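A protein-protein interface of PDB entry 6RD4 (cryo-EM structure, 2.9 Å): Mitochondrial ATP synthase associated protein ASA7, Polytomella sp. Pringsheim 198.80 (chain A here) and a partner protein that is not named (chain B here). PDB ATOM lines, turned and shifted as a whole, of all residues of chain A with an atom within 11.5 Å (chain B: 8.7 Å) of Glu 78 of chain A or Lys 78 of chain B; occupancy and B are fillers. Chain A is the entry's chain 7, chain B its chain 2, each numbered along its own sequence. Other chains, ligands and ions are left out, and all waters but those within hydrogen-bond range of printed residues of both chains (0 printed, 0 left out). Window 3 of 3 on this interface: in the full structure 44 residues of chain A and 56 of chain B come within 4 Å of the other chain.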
ATOM      1  N   LEU A  15      -3.074  -3.657 -16.818  1.00  0.00           N
ATOM      2  CA  LEU A  15      -2.746  -3.631 -18.227  1.00  0.00           C
ATOM      3  C   LEU A  15      -3.722  -2.769 -18.988  1.00  0.00           C
ATOM      4  O   LEU A  15      -4.851  -2.580 -18.559  1.00  0.00           O
ATOM      5  CB  LEU A  15      -2.734  -5.039 -18.797  1.00  0.00           C
ATOM      6  CG  LEU A  15      -1.356  -5.614 -19.050  1.00  0.00           C
ATOM      7  CD1 LEU A  15      -1.511  -6.959 -19.655  1.00  0.00           C
ATOM      8  CD2 LEU A  15      -0.617  -4.717 -20.000  1.00  0.00           C
ATOM      9  N   ILE A  74      -5.920 -11.734 -17.550  1.00  0.00           N
ATOM     10  CA  ILE A  74      -6.023 -12.716 -16.475  1.00  0.00           C
ATOM     11  C   ILE A  74      -6.464 -12.046 -15.184  1.00  0.00           C
ATOM     12  O   ILE A  74      -7.469 -12.444 -14.583  1.00  0.00           O
ATOM     13  CB  ILE A  74      -4.698 -13.469 -16.281  1.00  0.00           C
ATOM     14  CG1 ILE A  74      -4.419 -14.368 -17.474  1.00  0.00           C
ATOM     15  CG2 ILE A  74      -4.785 -14.333 -15.059  1.00  0.00           C
ATOM     16  CD1 ILE A  74      -5.391 -15.495 -17.601  1.00  0.00           C
ATOM     17  N   SER A  75      -5.717 -11.028 -14.752  1.00  0.00           N
ATOM     18  CA  SER A  75      -5.981 -10.225 -13.556  1.00  0.00           C
ATOM     19  C   SER A  75      -6.006 -11.093 -12.297  1.00  0.00           C
ATOM     20  O   SER A  75      -7.045 -11.368 -11.703  1.00  0.00           O
ATOM     21  CB  SER A  75      -7.257  -9.396 -13.695  1.00  0.00           C
ATOM     22  OG  SER A  75      -7.407  -8.564 -12.567  1.00  0.00           O
ATOM     23  N   LEU A  76      -4.810 -11.557 -11.957  1.00  0.00           N
ATOM     24  CA  LEU A  76      -4.595 -12.378 -10.780  1.00  0.00           C
ATOM     25  C   LEU A  76      -4.878 -11.595  -9.515  1.00  0.00           C
ATOM     26  O   LEU A  76      -4.677 -10.383  -9.450  1.00  0.00           O
ATOM     27  CB  LEU A  76      -3.163 -12.871 -10.755  1.00  0.00           C
ATOM     28  CG  LEU A  76      -2.814 -13.783 -11.897  1.00  0.00           C
ATOM     29  CD1 LEU A  76      -1.373 -13.979 -11.844  1.00  0.00           C
ATOM     30  CD2 LEU A  76      -3.521 -15.060 -11.669  1.00  0.00           C
ATOM     31  N   ALA A  77      -5.347 -12.301  -8.499  1.00  0.00           N
ATOM     32  CA  ALA A  77      -5.649 -11.660  -7.237  1.00  0.00           C
ATOM     33  C   ALA A  77      -5.488 -12.672  -6.132  1.00  0.00           C
ATOM     34  O   ALA A  77      -5.749 -13.857  -6.314  1.00  0.00           O
ATOM     35  CB  ALA A  77      -7.052 -11.087  -7.211  1.00  0.00           C
ATOM     36  N   GLU A  78      -5.079 -12.181  -4.977  1.00  0.00           N
ATOM     37  CA  GLU A  78      -4.601 -13.029  -3.910  1.00  0.00           C
ATOM     38  C   GLU A  78      -5.761 -13.491  -3.053  1.00  0.00           C
ATOM     39  O   GLU A  78      -6.601 -12.688  -2.650  1.00  0.00           O
ATOM     40  CB  GLU A  78      -3.584 -12.275  -3.072  1.00  0.00           C
ATOM     41  CG  GLU A  78      -2.505 -11.697  -3.922  1.00  0.00           C
ATOM     42  CD  GLU A  78      -1.364 -11.168  -3.127  1.00  0.00           C
ATOM     43  OE1 GLU A  78      -1.434 -11.230  -1.895  1.00  0.00           O
ATOM     44  OE2 GLU A  78      -0.386 -10.687  -3.722  1.00  0.00           O
ATOM     45  N   VAL A  79      -5.803 -14.787  -2.788  1.00  0.00           N
ATOM     46  CA  VAL A  79      -6.776 -15.361  -1.877  1.00  0.00           C
ATOM     47  C   VAL A  79      -6.116 -15.420  -0.512  1.00  0.00           C
ATOM     48  O   VAL A  79      -5.223 -16.230  -0.280  1.00  0.00           O
ATOM     49  CB  VAL A  79      -7.221 -16.746  -2.341  1.00  0.00           C
ATOM     50  CG1 VAL A  79      -8.109 -17.360  -1.316  1.00  0.00           C
ATOM     51  CG2 VAL A  79      -7.931 -16.621  -3.638  1.00  0.00           C
ATOM     52  N   ALA A  80      -6.542 -14.555   0.387  1.00  0.00           N
ATOM     53  CA  ALA A  80      -5.922 -14.441   1.689  1.00  0.00           C
ATOM     54  C   ALA A  80      -6.853 -14.996   2.744  1.00  0.00           C
ATOM     55  O   ALA A  80      -8.057 -15.107   2.532  1.00  0.00           O
ATOM     56  CB  ALA A  80      -5.579 -12.993   1.992  1.00  0.00           C
ATOM     57  N   ARG A  81      -6.275 -15.378   3.877  1.00  0.00           N
ATOM     58  CA  ARG A  81      -7.094 -15.912   4.951  1.00  0.00           C
ATOM     59  C   ARG A  81      -7.952 -14.825   5.551  1.00  0.00           C
ATOM     60  O   ARG A  81      -9.157 -14.999   5.727  1.00  0.00           O
ATOM     61  CB  ARG A  81      -6.230 -16.546   6.025  1.00  0.00           C
ATOM     62  CG  ARG A  81      -7.024 -16.969   7.206  1.00  0.00           C
ATOM     63  CD  ARG A  81      -6.272 -17.910   8.050  1.00  0.00           C
ATOM     64  NE  ARG A  81      -7.013 -18.249   9.250  1.00  0.00           N
ATOM     65  CZ  ARG A  81      -6.803 -17.677  10.421  1.00  0.00           C
ATOM     66  NH1 ARG A  81      -7.503 -18.039  11.475  1.00  0.00           N
ATOM     67  NH2 ARG A  81      -5.886 -16.738  10.532  1.00  0.00           N
ATOM     68  N   ILE A  82      -7.352 -13.685   5.844  1.00  0.00           N
ATOM     69  CA  ILE A  82      -8.067 -12.524   6.338  1.00  0.00           C
ATOM     70  C   ILE A  82      -8.006 -11.383   5.337  1.00  0.00           C
ATOM     71  O   ILE A  82      -9.024 -10.995   4.775  1.00  0.00           O
ATOM     72  CB  ILE A  82      -7.543 -12.103   7.721  1.00  0.00           C
ATOM     73  CG1 ILE A  82      -7.867 -13.205   8.710  1.00  0.00           C
ATOM     74  CG2 ILE A  82      -8.181 -10.837   8.150  1.00  0.00           C
ATOM     75  CD1 ILE A  82      -7.379 -12.960  10.060  1.00  0.00           C
ATOM     76  N   SER A  83      -6.817 -10.880   5.051  1.00  0.00           N
ATOM     77  CA  SER A  83      -6.654  -9.869   4.022  1.00  0.00           C
ATOM     78  C   SER A  83      -5.210  -9.906   3.573  1.00  0.00           C
ATOM     79  O   SER A  83      -4.392 -10.620   4.139  1.00  0.00           O
ATOM     80  CB  SER A  83      -7.051  -8.485   4.522  1.00  0.00           C
ATOM     81  OG  SER A  83      -6.362  -8.135   5.694  1.00  0.00           O
ATOM     82  N   VAL A  84      -4.916  -9.171   2.511  1.00  0.00           N
ATOM     83  CA  VAL A  84      -3.548  -9.081   2.033  1.00  0.00           C
ATOM     84  C   VAL A  84      -2.719  -8.214   2.952  1.00  0.00           C
ATOM     85  O   VAL A  84      -1.517  -8.432   3.100  1.00  0.00           O
ATOM     86  CB  VAL A  84      -3.549  -8.558   0.596  1.00  0.00           C
ATOM     87  CG1 VAL A  84      -2.218  -8.657   0.001  1.00  0.00           C
ATOM     88  CG2 VAL A  84      -4.464  -9.379  -0.208  1.00  0.00           C
ATOM     89  N   LEU A  85      -3.335  -7.233   3.595  1.00  0.00           N
ATOM     90  CA  LEU A  85      -2.620  -6.405   4.553  1.00  0.00           C
ATOM     91  C   LEU A  85      -2.218  -7.209   5.769  1.00  0.00           C
ATOM     92  O   LEU A  85      -1.065  -7.166   6.193  1.00  0.00           O
ATOM     93  CB  LEU A  85      -3.488  -5.237   4.973  1.00  0.00           C
ATOM     94  CG  LEU A  85      -2.991  -4.467   6.172  1.00  0.00           C
ATOM     95  CD1 LEU A  85      -1.817  -3.711   5.771  1.00  0.00           C
ATOM     96  CD2 LEU A  85      -4.036  -3.557   6.663  1.00  0.00           C
ATOM     97  N   HIS A  86      -3.162  -7.954   6.327  1.00  0.00           N
ATOM     98  CA  HIS A  86      -2.932  -8.742   7.522  1.00  0.00           C
ATOM     99  C   HIS A  86      -1.921  -9.837   7.284  1.00  0.00           C
ATOM    100  O   HIS A  86      -1.089 -10.103   8.143  1.00  0.00           O
ATOM    101  CB  HIS A  86      -4.255  -9.325   7.958  1.00  0.00           C
ATOM    102  CG  HIS A  86      -4.181 -10.173   9.174  1.00  0.00           C
ATOM    103  ND1 HIS A  86      -4.560  -9.717  10.410  1.00  0.00           N
ATOM    104  CD2 HIS A  86      -3.829 -11.466   9.341  1.00  0.00           C
ATOM    105  CE1 HIS A  86      -4.413 -10.683  11.290  1.00  0.00           C
ATOM    106  NE2 HIS A  86      -3.974 -11.755  10.666  1.00  0.00           N
ATOM    107  N   SER A  87      -1.957 -10.459   6.120  1.00  0.00           N
ATOM    108  CA  SER A  87      -1.025 -11.517   5.792  1.00  0.00           C
ATOM    109  C   SER A  87       0.375 -11.008   5.575  1.00  0.00           C
ATOM    110  O   SER A  87       1.310 -11.792   5.623  1.00  0.00           O
ATOM    111  CB  SER A  87      -1.496 -12.232   4.549  1.00  0.00           C
ATOM    112  OG  SER A  87      -2.682 -12.929   4.838  1.00  0.00           O
ATOM    113  N   SER A  88       0.541  -9.725   5.306  1.00  0.00           N
ATOM    114  CA  SER A  88       1.863  -9.158   5.140  1.00  0.00           C
ATOM    115  C   SER A  88       2.449  -8.720   6.455  1.00  0.00           C
ATOM    116  O   SER A  88       3.667  -8.626   6.584  1.00  0.00           O
ATOM    117  CB  SER A  88       1.791  -7.970   4.212  1.00  0.00           C
ATOM    118  OG  SER A  88       1.344  -6.866   4.945  1.00  0.00           O
ATOM    119  N   ILE A  89       1.596  -8.403   7.416  1.00  0.00           N
ATOM    120  CA  ILE A  89       2.039  -8.153   8.777  1.00  0.00           C
ATOM    121  C   ILE A  89       2.353  -9.459   9.465  1.00  0.00           C
ATOM    122  O   ILE A  89       3.362  -9.574  10.156  1.00  0.00           O
ATOM    123  CB  ILE A  89       0.966  -7.362   9.532  1.00  0.00           C
ATOM    124  CG1 ILE A  89       0.692  -6.050   8.827  1.00  0.00           C
ATOM    125  CG2 ILE A  89       1.406  -7.092  10.909  1.00  0.00           C
ATOM    126  CD1 ILE A  89      -0.373  -5.263   9.436  1.00  0.00           C
ATOM    127  N   ASN A  91       3.248 -12.216   7.989  1.00  0.00           N
ATOM    128  CA  ASN A  91       4.465 -12.747   7.410  1.00  0.00           C
ATOM    129  C   ASN A  91       5.682 -12.054   7.969  1.00  0.00           C
ATOM    130  O   ASN A  91       6.754 -12.645   8.018  1.00  0.00           O
ATOM    131  CB  ASN A  91       4.427 -12.603   5.907  1.00  0.00           C
ATOM    132  CG  ASN A  91       5.602 -13.190   5.249  1.00  0.00           C
ATOM    133  OD1 ASN A  91       5.826 -14.379   5.320  1.00  0.00           O
ATOM    134  ND2 ASN A  91       6.376 -12.361   4.588  1.00  0.00           N
ATOM    135  N   ARG B  41      -5.504 -20.144 -14.485  1.00  0.00           N
ATOM    136  CA  ARG B  41      -5.098 -18.940 -13.788  1.00  0.00           C
ATOM    137  C   ARG B  41      -4.177 -19.242 -12.630  1.00  0.00           C
ATOM    138  O   ARG B  41      -3.330 -18.414 -12.296  1.00  0.00           O
ATOM    139  CB  ARG B  41      -6.312 -18.196 -13.264  1.00  0.00           C
ATOM    140  CG  ARG B  41      -7.339 -17.902 -14.292  1.00  0.00           C
ATOM    141  CD  ARG B  41      -8.588 -17.422 -13.617  1.00  0.00           C
ATOM    142  NE  ARG B  41      -8.298 -16.397 -12.633  1.00  0.00           N
ATOM    143  CZ  ARG B  41      -8.234 -15.106 -12.917  1.00  0.00           C
ATOM    144  NH1 ARG B  41      -7.969 -14.227 -11.969  1.00  0.00           N
ATOM    145  NH2 ARG B  41      -8.444 -14.697 -14.157  1.00  0.00           N
ATOM    146  N   ARG B  42      -4.337 -20.406 -11.999  1.00  0.00           N
ATOM    147  CA  ARG B  42      -3.506 -20.738 -10.852  1.00  0.00           C
ATOM    148  C   ARG B  42      -2.074 -21.006 -11.278  1.00  0.00           C
ATOM    149  O   ARG B  42      -1.140 -20.649 -10.564  1.00  0.00           O
ATOM    150  CB  ARG B  42      -4.097 -21.931 -10.118  1.00  0.00           C
ATOM    151  CG  ARG B  42      -3.354 -22.380  -8.891  1.00  0.00           C
ATOM    152  CD  ARG B  42      -3.055 -21.251  -7.943  1.00  0.00           C
ATOM    153  NE  ARG B  42      -2.281 -21.697  -6.799  1.00  0.00           N
ATOM    154  CZ  ARG B  42      -1.339 -20.971  -6.223  1.00  0.00           C
ATOM    155  NH1 ARG B  42      -1.052 -19.779  -6.687  1.00  0.00           N
ATOM    156  NH2 ARG B  42      -0.679 -21.440  -5.189  1.00  0.00           N
ATOM    157  N   GLY B  45      -0.553 -17.911 -11.595  1.00  0.00           N
ATOM    158  CA  GLY B  45      -0.338 -17.360 -10.277  1.00  0.00           C
ATOM    159  C   GLY B  45       0.887 -17.913  -9.595  1.00  0.00           C
ATOM    160  O   GLY B  45       1.545 -17.203  -8.840  1.00  0.00           O
ATOM    161  N   LEU B  48       3.949 -15.923 -11.097  1.00  0.00           N
ATOM    162  CA  LEU B  48       4.176 -14.589 -10.575  1.00  0.00           C
ATOM    163  C   LEU B  48       4.424 -14.596  -9.080  1.00  0.00           C
ATOM    164  O   LEU B  48       4.927 -13.609  -8.550  1.00  0.00           O
ATOM    165  CB  LEU B  48       3.007 -13.676 -10.915  1.00  0.00           C
ATOM    166  CG  LEU B  48       2.826 -13.342 -12.390  1.00  0.00           C
ATOM    167  CD1 LEU B  48       1.796 -12.283 -12.546  1.00  0.00           C
ATOM    168  CD2 LEU B  48       4.114 -12.889 -13.011  1.00  0.00           C
ATOM    169  N   GLU B  49       4.087 -15.672  -8.385  1.00  0.00           N
ATOM    170  CA  GLU B  49       4.487 -15.789  -6.991  1.00  0.00           C
ATOM    171  C   GLU B  49       5.981 -15.999  -6.866  1.00  0.00           C
ATOM    172  O   GLU B  49       6.613 -15.451  -5.963  1.00  0.00           O
ATOM    173  CB  GLU B  49       3.750 -16.935  -6.333  1.00  0.00           C
ATOM    174  CG  GLU B  49       2.473 -16.528  -5.715  1.00  0.00           C
ATOM    175  CD  GLU B  49       1.908 -17.617  -4.868  1.00  0.00           C
ATOM    176  OE1 GLU B  49       1.860 -18.767  -5.342  1.00  0.00           O
ATOM    177  OE2 GLU B  49       1.525 -17.327  -3.718  1.00  0.00           O
ATOM    178  N   ALA B  51       8.022 -15.043  -9.213  1.00  0.00           N
ATOM    179  CA  ALA B  51       8.652 -13.906  -9.859  1.00  0.00           C
ATOM    180  C   ALA B  51       8.884 -12.765  -8.896  1.00  0.00           C
ATOM    181  O   ALA B  51       9.715 -11.902  -9.171  1.00  0.00           O
ATOM    182  CB  ALA B  51       7.807 -13.433 -11.026  1.00  0.00           C
ATOM    183  N   GLY B  52       8.163 -12.723  -7.792  1.00  0.00           N
ATOM    184  CA  GLY B  52       8.464 -11.754  -6.770  1.00  0.00           C
ATOM    185  C   GLY B  52       9.516 -12.285  -5.828  1.00  0.00           C
ATOM    186  O   GLY B  52      10.324 -11.526  -5.291  1.00  0.00           O
ATOM    187  N   ALA B  53       9.524 -13.599  -5.630  1.00  0.00           N
ATOM    188  CA  ALA B  53      10.497 -14.221  -4.752  1.00  0.00           C
ATOM    189  C   ALA B  53      11.886 -14.275  -5.350  1.00  0.00           C
ATOM    190  O   ALA B  53      12.855 -14.364  -4.598  1.00  0.00           O
ATOM    191  CB  ALA B  53      10.057 -15.636  -4.407  1.00  0.00           C
ATOM    192  N   GLU B  75      -2.070  -9.665 -15.525  1.00  0.00           N
ATOM    193  CA  GLU B  75      -1.732  -8.494 -14.743  1.00  0.00           C
ATOM    194  C   GLU B  75      -1.832  -8.824 -13.269  1.00  0.00           C
ATOM    195  O   GLU B  75      -2.798  -9.443 -12.824  1.00  0.00           O
ATOM    196  CB  GLU B  75      -2.611  -7.302 -15.099  1.00  0.00           C
ATOM    197  CG  GLU B  75      -4.063  -7.602 -15.158  1.00  0.00           C
ATOM    198  CD  GLU B  75      -4.892  -6.397 -15.479  1.00  0.00           C
ATOM    199  OE1 GLU B  75      -4.311  -5.312 -15.654  1.00  0.00           O
ATOM    200  OE2 GLU B  75      -6.129  -6.527 -15.559  1.00  0.00           O
ATOM    201  N   HIS B  76      -0.795  -8.458 -12.538  1.00  0.00           N
ATOM    202  CA  HIS B  76      -0.831  -8.431 -11.089  1.00  0.00           C
ATOM    203  C   HIS B  76       0.059  -7.263 -10.730  1.00  0.00           C
ATOM    204  O   HIS B  76       1.256  -7.331 -10.988  1.00  0.00           O
ATOM    205  CB  HIS B  76      -0.321  -9.725 -10.486  1.00  0.00           C
ATOM    206  CG  HIS B  76      -0.365  -9.746  -8.994  1.00  0.00           C
ATOM    207  ND1 HIS B  76       0.760  -9.890  -8.221  1.00  0.00           N
ATOM    208  CD2 HIS B  76      -1.398  -9.617  -8.135  1.00  0.00           C
ATOM    209  CE1 HIS B  76       0.423  -9.858  -6.947  1.00  0.00           C
ATOM    210  NE2 HIS B  76      -0.881  -9.689  -6.869  1.00  0.00           N
ATOM    211  N   PHE B  77      -0.520  -6.201 -10.171  1.00  0.00           N
ATOM    212  CA  PHE B  77       0.231  -4.968 -10.012  1.00  0.00           C
ATOM    213  C   PHE B  77       1.354  -5.101  -9.015  1.00  0.00           C
ATOM    214  O   PHE B  77       2.396  -4.485  -9.203  1.00  0.00           O
ATOM    215  CB  PHE B  77      -0.670  -3.825  -9.577  1.00  0.00           C
ATOM    216  CG  PHE B  77       0.030  -2.509  -9.524  1.00  0.00           C
ATOM    217  CD1 PHE B  77       0.344  -1.840 -10.677  1.00  0.00           C
ATOM    218  CD2 PHE B  77       0.391  -1.952  -8.327  1.00  0.00           C
ATOM    219  CE1 PHE B  77       0.996  -0.648 -10.623  1.00  0.00           C
ATOM    220  CE2 PHE B  77       1.042  -0.758  -8.277  1.00  0.00           C
ATOM    221  CZ  PHE B  77       1.343  -0.111  -9.421  1.00  0.00           C
ATOM    222  N   LYS B  78       1.179  -5.902  -7.972  1.00  0.00           N
ATOM    223  CA  LYS B  78       2.208  -6.005  -6.950  1.00  0.00           C
ATOM    224  C   LYS B  78       3.447  -6.694  -7.482  1.00  0.00           C
ATOM    225  O   LYS B  78       4.566  -6.301  -7.159  1.00  0.00           O
ATOM    226  CB  LYS B  78       1.661  -6.752  -5.750  1.00  0.00           C
ATOM    227  CG  LYS B  78       2.641  -6.887  -4.637  1.00  0.00           C
ATOM    228  CD  LYS B  78       2.167  -7.850  -3.621  1.00  0.00           C
ATOM    229  CE  LYS B  78       3.250  -8.087  -2.623  1.00  0.00           C
ATOM    230  NZ  LYS B  78       4.546  -8.206  -3.326  1.00  0.00           N
ATOM    231  N   THR B  79       3.270  -7.692  -8.330  1.00  0.00           N
ATOM    232  CA  THR B  79       4.407  -8.434  -8.847  1.00  0.00           C
ATOM    233  C   THR B  79       5.161  -7.645  -9.894  1.00  0.00           C
ATOM    234  O   THR B  79       6.391  -7.595  -9.866  1.00  0.00           O
ATOM    235  CB  THR B  79       3.939  -9.742  -9.441  1.00  0.00           C
ATOM    236  OG1 THR B  79       3.128 -10.422  -8.481  1.00  0.00           O
ATOM    237  CG2 THR B  79       5.115 -10.579  -9.791  1.00  0.00           C
ATOM    238  N   VAL B  80       4.438  -7.012 -10.809  1.00  0.00           N
ATOM    239  CA  VAL B  80       5.071  -6.309 -11.910  1.00  0.00           C
ATOM    240  C   VAL B  80       5.722  -5.024 -11.425  1.00  0.00           C
ATOM    241  O   VAL B  80       6.809  -4.665 -11.876  1.00  0.00           O
ATOM    242  CB  VAL B  80       4.038  -6.062 -13.013  1.00  0.00           C
ATOM    243  CG1 VAL B  80       4.649  -5.383 -14.181  1.00  0.00           C
ATOM    244  CG2 VAL B  80       3.467  -7.362 -13.439  1.00  0.00           C
ATOM    245  N   ALA B  81       5.102  -4.329 -10.477  1.00  0.00           N
ATOM    246  CA  ALA B  81       5.676  -3.067 -10.036  1.00  0.00           C
ATOM    247  C   ALA B  81       6.900  -3.240  -9.173  1.00  0.00           C
ATOM    248  O   ALA B  81       7.666  -2.291  -9.025  1.00  0.00           O
ATOM    249  CB  ALA B  81       4.664  -2.234  -9.280  1.00  0.00           C
ATOM    250  N   GLU B  82       7.103  -4.413  -8.605  1.00  0.00           N
ATOM    251  CA  GLU B  82       8.321  -4.701  -7.879  1.00  0.00           C
ATOM    252  C   GLU B  82       9.388  -5.292  -8.772  1.00  0.00           C
ATOM    253  O   GLU B  82      10.516  -5.476  -8.319  1.00  0.00           O
ATOM    254  CB  GLU B  82       8.020  -5.641  -6.728  1.00  0.00           C
ATOM    255  CG  GLU B  82       7.160  -4.995  -5.691  1.00  0.00           C
ATOM    256  CD  GLU B  82       7.036  -5.809  -4.446  1.00  0.00           C
ATOM    257  OE1 GLU B  82       6.710  -5.232  -3.396  1.00  0.00           O
ATOM    258  OE2 GLU B  82       7.269  -7.029  -4.505  1.00  0.00           O
ATOM    259  N   LEU B  83       9.060  -5.588 -10.026  1.00  0.00           N
ATOM    260  CA  LEU B  83      10.048  -5.899 -11.045  1.00  0.00           C
ATOM    261  C   LEU B  83      10.689  -4.656 -11.616  1.00  0.00           C
ATOM    262  O   LEU B  83      11.563  -4.767 -12.471  1.00  0.00           O
ATOM    263  CB  LEU B  83       9.423  -6.691 -12.185  1.00  0.00           C
ATOM    264  CG  LEU B  83       8.990  -8.117 -11.917  1.00  0.00           C
ATOM    265  CD1 LEU B  83       8.274  -8.658 -13.101  1.00  0.00           C
ATOM    266  CD2 LEU B  83      10.185  -8.930 -11.626  1.00  0.00           C
ATOM    267  N   ALA B  84      10.253  -3.481 -11.196  1.00  0.00           N
ATOM    268  CA  ALA B  84      10.922  -2.244 -11.543  1.00  0.00           C
ATOM    269  C   ALA B  84      12.122  -1.975 -10.663  1.00  0.00           C
ATOM    270  O   ALA B  84      12.809  -0.977 -10.873  1.00  0.00           O
ATOM    271  CB  ALA B  84       9.950  -1.079 -11.441  1.00  0.00           C
ATOM    272  N   ALA B 109       1.554  -1.631 -17.570  1.00  0.00           N
ATOM    273  CA  ALA B 109       0.883  -2.089 -16.369  1.00  0.00           C
ATOM    274  C   ALA B 109       0.588  -0.966 -15.399  1.00  0.00           C
ATOM    275  O   ALA B 109      -0.121  -1.191 -14.419  1.00  0.00           O
ATOM    276  CB  ALA B 109       1.719  -3.152 -15.672  1.00  0.00           C
ATOM    277  N   VAL B 111       2.906   1.070 -13.719  1.00  0.00           N
ATOM    278  CA  VAL B 111       3.837   1.160 -12.606  1.00  0.00           C
ATOM    279  C   VAL B 111       4.295   2.599 -12.465  1.00  0.00           C
ATOM    280  O   VAL B 111       4.959   3.144 -13.352  1.00  0.00           O
ATOM    281  CB  VAL B 111       5.020   0.220 -12.829  1.00  0.00           C
ATOM    282  CG1 VAL B 111       6.009   0.340 -11.731  1.00  0.00           C
ATOM    283  CG2 VAL B 111       4.520  -1.169 -12.962  1.00  0.00           C
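The guanidinium group (NH2) of Arg 41 of chain B lies within hydrogen-bond range of the backbone carbonyl oxygen (O) of Ile 74 of chain A (2.5 Å). O of Ser 75 of chain A sits at hydrogen-bond distance from NH1 of Arg 41 of chain B, 3.0 Å away. The backbone carbonyl oxygen (O) of Glu 75 of chain B sits at hydrogen-bond distance from the backbone NH (N) of Leu 76 of chain A (3.0 Å). A ring nitrogen (NE2) of His 76 of chain B sits at hydrogen-bond distance from the side-chain carboxylate of Glu 78 of chain A, 3.3 Å away. N of Leu 15 of chain A sits close to OE1 of Glu 75 of chain B (2.4 Å).
A ring nitrogen (ND1) of His 76 of chain B lies within hydrogen-bond range of the side-chain hydroxyl (OG1) of Thr 79 of chain B, at 2.4 Å. OE2 of Glu 82 of chain B lies within salt-bridge range of NZ of Lys 78 of chain B (3.2 Å).
Among the printed residues, merely in contact across the chains: Ser 75 of chain A with Glu 75 of chain B (3.4 Å), Leu 76 of chain A with Arg 41 of chain B (3.4 Å), Leu 76 of chain A with Gly 45 of chain B (3.9 Å), Leu 76 of chain A with Leu 48 of chain B (3.7 Å), Leu 76 of chain A with His 76 of chain B (3.6 Å) and Glu 78 of chain A with Lys 78 of chain B (3.8 Å).
Of the printed residues of chain B, Leu 15 of chain A touches Glu 75. No residue of chain B comes within 4 Å of Ala 77 of chain A. Glu 78 of chain A touches just these residues of chain B: His 76 (3.3 Å) and Lys 78 (3.8 Å). Of the printed residues of chain A, Leu 48 of chain B touches Leu 76. Glu 49 of chain B touches none of the printed residues of chain A. No residue of chain A comes within 4 Å of Gly 52 of chain B. Of the printed residues of chain A, Glu 75 of chain B touches Leu 15, Ser 75 and Leu 76. His 76 of chain B touches just these residues of chain A: Leu 76 (3.6 Å) and Glu 78 (3.3 Å). No residue of chain A comes within 4 Å of Phe 77 of chain B. Of the printed residues of chain A, Lys 78 of chain B touches Glu 78. No residue of chain A comes within 4 Å of Thr 79 of chain B. No residue of chain A comes within 4 Å of Val 80 of chain B. Ala 81 of chain B touches none of the printed residues of chain A. No residue of chain A comes within 4 Å of Glu 82 of chain B. Ala 109 of chain B touches none of the printed residues of chain A. The nearest residue of chain B that does not touch Glu 78 of chain A is Thr 79 of chain B (5.9 Å).
Of the 20 printed residues of chain B, 6 touch a printed residue of chain A. Hydrophobic or aromatic side chains of chain B within 4 Å of the printed part of chain A: Leu 48 and His 76. Printed residues of chain A that touch a printed residue of chain B: Leu 15, Ile 74, Ser 75, Leu 76 and Glu 78.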
